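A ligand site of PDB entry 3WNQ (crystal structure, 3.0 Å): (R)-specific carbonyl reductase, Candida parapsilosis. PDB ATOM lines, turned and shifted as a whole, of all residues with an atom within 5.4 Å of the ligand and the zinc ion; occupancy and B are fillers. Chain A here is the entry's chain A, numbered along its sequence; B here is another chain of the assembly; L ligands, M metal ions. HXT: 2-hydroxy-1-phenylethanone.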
ATOM      1  N   LEU A  48      33.229  -9.390  -2.815  1.00  0.00           N
ATOM      2  CA  LEU A  48      33.653  -8.806  -1.588  1.00  0.00           C
ATOM      3  C   LEU A  48      34.410  -7.538  -1.879  1.00  0.00           C
ATOM      4  O   LEU A  48      35.361  -7.555  -2.663  1.00  0.00           O
ATOM      5  CB  LEU A  48      34.585  -9.784  -0.891  1.00  0.00           C
ATOM      6  CG  LEU A  48      35.388  -9.083   0.186  1.00  0.00           C
ATOM      7  CD1 LEU A  48      34.389  -8.392   1.168  1.00  0.00           C
ATOM      8  CD2 LEU A  48      36.313 -10.091   0.860  1.00  0.00           C
ATOM      9  N   CYS A  49      34.013  -6.450  -1.227  1.00  0.00           N
ATOM     10  CA  CYS A  49      34.712  -5.188  -1.404  1.00  0.00           C
ATOM     11  C   CYS A  49      34.885  -4.464  -0.077  1.00  0.00           C
ATOM     12  O   CYS A  49      34.342  -4.888   0.958  1.00  0.00           O
ATOM     13  CB  CYS A  49      33.966  -4.295  -2.402  1.00  0.00           C
ATOM     14  SG  CYS A  49      32.611  -3.404  -1.738  1.00  0.00           S
ATOM     15  N   SER A  51      33.570  -1.945   1.235  1.00  0.00           N
ATOM     16  CA  SER A  51      32.314  -1.625   1.950  1.00  0.00           C
ATOM     17  C   SER A  51      32.066  -2.661   3.038  1.00  0.00           C
ATOM     18  O   SER A  51      31.890  -2.319   4.188  1.00  0.00           O
ATOM     19  CB  SER A  51      31.115  -1.612   1.020  1.00  0.00           C
ATOM     20  OG  SER A  51      30.955  -0.346   0.437  1.00  0.00           O
ATOM     21  N   ASP A  52      32.068  -3.938   2.647  1.00  0.00           N
ATOM     22  CA  ASP A  52      31.841  -5.026   3.566  1.00  0.00           C
ATOM     23  C   ASP A  52      32.687  -4.878   4.854  1.00  0.00           C
ATOM     24  O   ASP A  52      32.205  -5.126   5.958  1.00  0.00           O
ATOM     25  CB  ASP A  52      32.095  -6.367   2.844  1.00  0.00           C
ATOM     26  CG  ASP A  52      30.907  -6.793   1.946  1.00  0.00           C
ATOM     27  OD1 ASP A  52      29.719  -6.767   2.419  1.00  0.00           O
ATOM     28  OD2 ASP A  52      31.176  -7.179   0.777  1.00  0.00           O
ATOM     29  N   LEU A  60      30.129   0.478  10.518  1.00  0.00           N
ATOM     30  CA  LEU A  60      29.147   1.135   9.718  1.00  0.00           C
ATOM     31  C   LEU A  60      27.815   0.433  10.109  1.00  0.00           C
ATOM     32  O   LEU A  60      27.684  -0.786   9.987  1.00  0.00           O
ATOM     33  CB  LEU A  60      29.503   0.966   8.236  1.00  0.00           C
ATOM     34  CG  LEU A  60      28.435   1.432   7.221  1.00  0.00           C
ATOM     35  CD1 LEU A  60      28.050   2.898   7.398  1.00  0.00           C
ATOM     36  CD2 LEU A  60      28.932   1.200   5.875  1.00  0.00           C
ATOM     37  N   HIS A  70      26.904  -7.860  -0.948  1.00  0.00           N
ATOM     38  CA  HIS A  70      25.929  -7.201  -1.785  1.00  0.00           C
ATOM     39  C   HIS A  70      26.189  -7.369  -3.282  1.00  0.00           C
ATOM     40  O   HIS A  70      25.322  -7.073  -4.143  1.00  0.00           O
ATOM     41  CB  HIS A  70      26.009  -5.767  -1.450  1.00  0.00           C
ATOM     42  CG  HIS A  70      27.405  -5.325  -1.252  1.00  0.00           C
ATOM     43  ND1 HIS A  70      28.163  -5.731  -0.173  1.00  0.00           N
ATOM     44  CD2 HIS A  70      28.224  -4.571  -2.030  1.00  0.00           C
ATOM     45  CE1 HIS A  70      29.389  -5.255  -0.302  1.00  0.00           C
ATOM     46  NE2 HIS A  70      29.456  -4.544  -1.415  1.00  0.00           N
ATOM     47  N   GLU A  71      27.392  -7.817  -3.587  1.00  0.00           N
ATOM     48  CA  GLU A  71      27.756  -7.989  -4.973  1.00  0.00           C
ATOM     49  C   GLU A  71      27.321  -9.385  -5.277  1.00  0.00           C
ATOM     50  O   GLU A  71      28.092 -10.286  -5.233  1.00  0.00           O
ATOM     51  CB  GLU A  71      29.252  -7.802  -5.097  1.00  0.00           C
ATOM     52  CG  GLU A  71      29.765  -6.740  -4.132  1.00  0.00           C
ATOM     53  CD  GLU A  71      30.922  -5.964  -4.664  1.00  0.00           C
ATOM     54  OE1 GLU A  71      31.672  -6.470  -5.543  1.00  0.00           O
ATOM     55  OE2 GLU A  71      31.098  -4.826  -4.174  1.00  0.00           O
ATOM     56  N   TRP A 121      19.139  -3.119   2.184  1.00  0.00           N
ATOM     57  CA  TRP A 121      20.004  -3.354   1.041  1.00  0.00           C
ATOM     58  C   TRP A 121      20.474  -4.783   1.073  1.00  0.00           C
ATOM     59  O   TRP A 121      20.672  -5.315   2.137  1.00  0.00           O
ATOM     60  CB  TRP A 121      21.230  -2.455   1.125  1.00  0.00           C
ATOM     61  CG  TRP A 121      20.908  -1.029   1.207  1.00  0.00           C
ATOM     62  CD1 TRP A 121      19.729  -0.454   0.896  1.00  0.00           C
ATOM     63  CD2 TRP A 121      21.803   0.029   1.498  1.00  0.00           C
ATOM     64  NE1 TRP A 121      19.829   0.905   0.973  1.00  0.00           N
ATOM     65  CE2 TRP A 121      21.106   1.222   1.349  1.00  0.00           C
ATOM     66  CE3 TRP A 121      23.135   0.096   1.882  1.00  0.00           C
ATOM     67  CZ2 TRP A 121      21.698   2.473   1.554  1.00  0.00           C
ATOM     68  CZ3 TRP A 121      23.713   1.343   2.088  1.00  0.00           C
ATOM     69  CH2 TRP A 121      23.002   2.507   1.924  1.00  0.00           C
ATOM     70  N   LEU A 124      23.437  -5.785   3.499  1.00  0.00           N
ATOM     71  CA  LEU A 124      23.734  -4.530   4.210  1.00  0.00           C
ATOM     72  C   LEU A 124      22.407  -4.004   4.808  1.00  0.00           C
ATOM     73  O   LEU A 124      22.036  -2.824   4.671  1.00  0.00           O
ATOM     74  CB  LEU A 124      24.321  -3.498   3.235  1.00  0.00           C
ATOM     75  CG  LEU A 124      25.586  -3.901   2.484  1.00  0.00           C
ATOM     76  CD1 LEU A 124      25.843  -2.950   1.389  1.00  0.00           C
ATOM     77  CD2 LEU A 124      26.779  -3.971   3.449  1.00  0.00           C
ATOM     78  N   ASP A 159      28.908  -3.723  -8.071  1.00  0.00           N
ATOM     79  CA  ASP A 159      29.337  -2.572  -7.325  1.00  0.00           C
ATOM     80  C   ASP A 159      30.520  -1.995  -8.097  1.00  0.00           C
ATOM     81  O   ASP A 159      30.505  -0.856  -8.586  1.00  0.00           O
ATOM     82  CB  ASP A 159      29.800  -2.948  -5.916  1.00  0.00           C
ATOM     83  CG  ASP A 159      30.139  -1.738  -5.059  1.00  0.00           C
ATOM     84  OD1 ASP A 159      30.772  -0.763  -5.548  1.00  0.00           O
ATOM     85  OD2 ASP A 159      29.781  -1.745  -3.862  1.00  0.00           O
ATOM     86  N   THR A 163      28.765   1.107  -9.686  1.00  0.00           N
ATOM     87  CA  THR A 163      28.939   2.411  -9.063  1.00  0.00           C
ATOM     88  C   THR A 163      29.504   3.472  -9.989  1.00  0.00           C
ATOM     89  O   THR A 163      28.887   4.560 -10.098  1.00  0.00           O
ATOM     90  CB  THR A 163      29.795   2.366  -7.784  1.00  0.00           C
ATOM     91  OG1 THR A 163      29.092   1.591  -6.810  1.00  0.00           O
ATOM     92  CG2 THR A 163      29.983   3.777  -7.216  1.00  0.00           C
ATOM     93  N   PHE A 290      25.565   7.747  -5.851  1.00  0.00           N
ATOM     94  CA  PHE A 290      25.694   6.593  -4.947  1.00  0.00           C
ATOM     95  C   PHE A 290      25.306   5.242  -5.567  1.00  0.00           C
ATOM     96  O   PHE A 290      24.143   5.015  -5.921  1.00  0.00           O
ATOM     97  CB  PHE A 290      24.816   6.874  -3.743  1.00  0.00           C
ATOM     98  CG  PHE A 290      24.596   5.709  -2.876  1.00  0.00           C
ATOM     99  CD1 PHE A 290      25.647   5.145  -2.160  1.00  0.00           C
ATOM    100  CD2 PHE A 290      23.352   5.139  -2.797  1.00  0.00           C
ATOM    101  CE1 PHE A 290      25.458   4.002  -1.363  1.00  0.00           C
ATOM    102  CE2 PHE A 290      23.136   3.960  -1.985  1.00  0.00           C
ATOM    103  CZ  PHE A 290      24.194   3.397  -1.276  1.00  0.00           C
ATOM    104  N   TRP A 291      26.275   4.342  -5.678  1.00  0.00           N
ATOM    105  CA  TRP A 291      25.990   3.040  -6.259  1.00  0.00           C
ATOM    106  C   TRP A 291      25.283   3.182  -7.610  1.00  0.00           C
ATOM    107  O   TRP A 291      25.778   3.967  -8.456  1.00  0.00           O
ATOM    108  CB  TRP A 291      25.108   2.250  -5.315  1.00  0.00           C
ATOM    109  CG  TRP A 291      25.480   0.778  -5.228  1.00  0.00           C
ATOM    110  CD1 TRP A 291      26.062   0.002  -6.217  1.00  0.00           C
ATOM    111  CD2 TRP A 291      25.172  -0.125  -4.141  1.00  0.00           C
ATOM    112  NE1 TRP A 291      26.120  -1.321  -5.817  1.00  0.00           N
ATOM    113  CE2 TRP A 291      25.583  -1.422  -4.549  1.00  0.00           C
ATOM    114  CE3 TRP A 291      24.584   0.033  -2.892  1.00  0.00           C
ATOM    115  CZ2 TRP A 291      25.417  -2.545  -3.741  1.00  0.00           C
ATOM    116  CZ3 TRP A 291      24.417  -1.083  -2.100  1.00  0.00           C
ATOM    117  CH2 TRP A 291      24.835  -2.352  -2.529  1.00  0.00           C
ATOM    118  N   ARG A 336      39.392  -7.558  -7.211  1.00  0.00           N
ATOM    119  CA  ARG A 336      38.118  -8.095  -6.784  1.00  0.00           C
ATOM    120  C   ARG A 336      38.142  -9.637  -6.601  1.00  0.00           C
ATOM    121  O   ARG A 336      38.764 -10.346  -7.386  1.00  0.00           O
ATOM    122  CB  ARG A 336      37.042  -7.654  -7.807  1.00  0.00           C
ATOM    123  CG  ARG A 336      36.620  -6.238  -7.657  1.00  0.00           C
ATOM    124  CD  ARG A 336      36.086  -6.089  -6.263  1.00  0.00           C
ATOM    125  NE  ARG A 336      35.901  -4.706  -5.890  1.00  0.00           N
ATOM    126  CZ  ARG A 336      34.719  -4.203  -5.561  1.00  0.00           C
ATOM    127  NH1 ARG A 336      33.651  -5.008  -5.578  1.00  0.00           N
ATOM    128  NH2 ARG A 336      34.608  -2.901  -5.242  1.00  0.00           N
ATOM    129  N   LEU B 281      25.159   9.869  -0.416  1.00  0.00           N
ATOM    130  CA  LEU B 281      24.103   8.913  -0.174  1.00  0.00           C
ATOM    131  C   LEU B 281      22.715   9.367  -0.637  1.00  0.00           C
ATOM    132  O   LEU B 281      21.868   8.532  -0.945  1.00  0.00           O
ATOM    133  CB  LEU B 281      24.061   8.558   1.311  1.00  0.00           C
ATOM    134  CG  LEU B 281      22.869   7.669   1.702  1.00  0.00           C
ATOM    135  CD1 LEU B 281      23.159   6.255   1.381  1.00  0.00           C
ATOM    136  CD2 LEU B 281      22.512   7.847   3.138  1.00  0.00           C
HETATM  137  CAF HXT L   1      28.574   3.346   0.255  1.00  0.00           C
HETATM  138  CAD HXT L   1      28.315   4.304   1.228  1.00  0.00           C
HETATM  139  CAC HXT L   1      27.666   3.920   2.399  1.00  0.00           C
HETATM  140  CAE HXT L   1      27.284   2.596   2.578  1.00  0.00           C
HETATM  141  CAG HXT L   1      27.534   1.644   1.595  1.00  0.00           C
HETATM  142  CAJ HXT L   1      28.155   2.026   0.408  1.00  0.00           C
HETATM  143  CAI HXT L   1      28.195   1.142  -0.665  1.00  0.00           C
HETATM  144  OAA HXT L   1      27.954  -0.053  -0.510  1.00  0.00           O
HETATM  145  CAH HXT L   1      28.378   1.752  -2.066  1.00  0.00           C
HETATM  146  OAB HXT L   1      29.195   0.924  -2.894  1.00  0.00           O
HETATM  147 ZN    ZN M   1      30.916  -3.668  -2.866  1.00  0.00          ZN
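An oxygen (OAB) of the ligand lies close to the side-chain carboxylate of Asp 159 (2.9 Å). The side-chain hydroxyl (OG) of Ser 51 is in hydrogen-bond range of an oxygen (OAA) of the ligand.
The guanidinium group (NH1) of Arg 336 lies within salt-bridge range of the side-chain carboxylate (OE1) of Glu 71. The side-chain sulfur (SG) of Cys 49 lies close to the backbone NH (N) of Ser 51 (3.4 Å). The side-chain carboxylate of Asp 52 sits close to a ring nitrogen (ND1) of His 70 (3.2 Å). OD1 of Asp 159 lies within hydrogen-bond range of OG1 of Thr 163, 3.2 Å away.
CD2 of Leu 60 touches CAE of the ligand, 3.9 Å away. Trp 121 touches the ligand (CZ3 to CAE, 3.8 Å). Thr 163 touches the ligand (OG1 to OAB, 3.97 Å). Phe 290 touches the ligand. Hydrophobic or aromatic side chains within 4 Å of the ligand: Leu 60, Trp 121 and Phe 290. The nearest printed residue that does not touch the ligand is Trp 291 (4.01 Å).
Within 4 Å of the zinc ion: Cys 49, His 70, Glu 71 and Asp 159.
The side-chain carboxylate (OE2) of Glu 71 binds the zinc ion. The zinc ion is bound by SG of Cys 49 (2.1 Å). NE2 of His 70 binds the zinc ion (2.2 Å). The zinc ion is bound by OD2 of Asp 159. The zinc ion has four donor atoms within binding distance.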
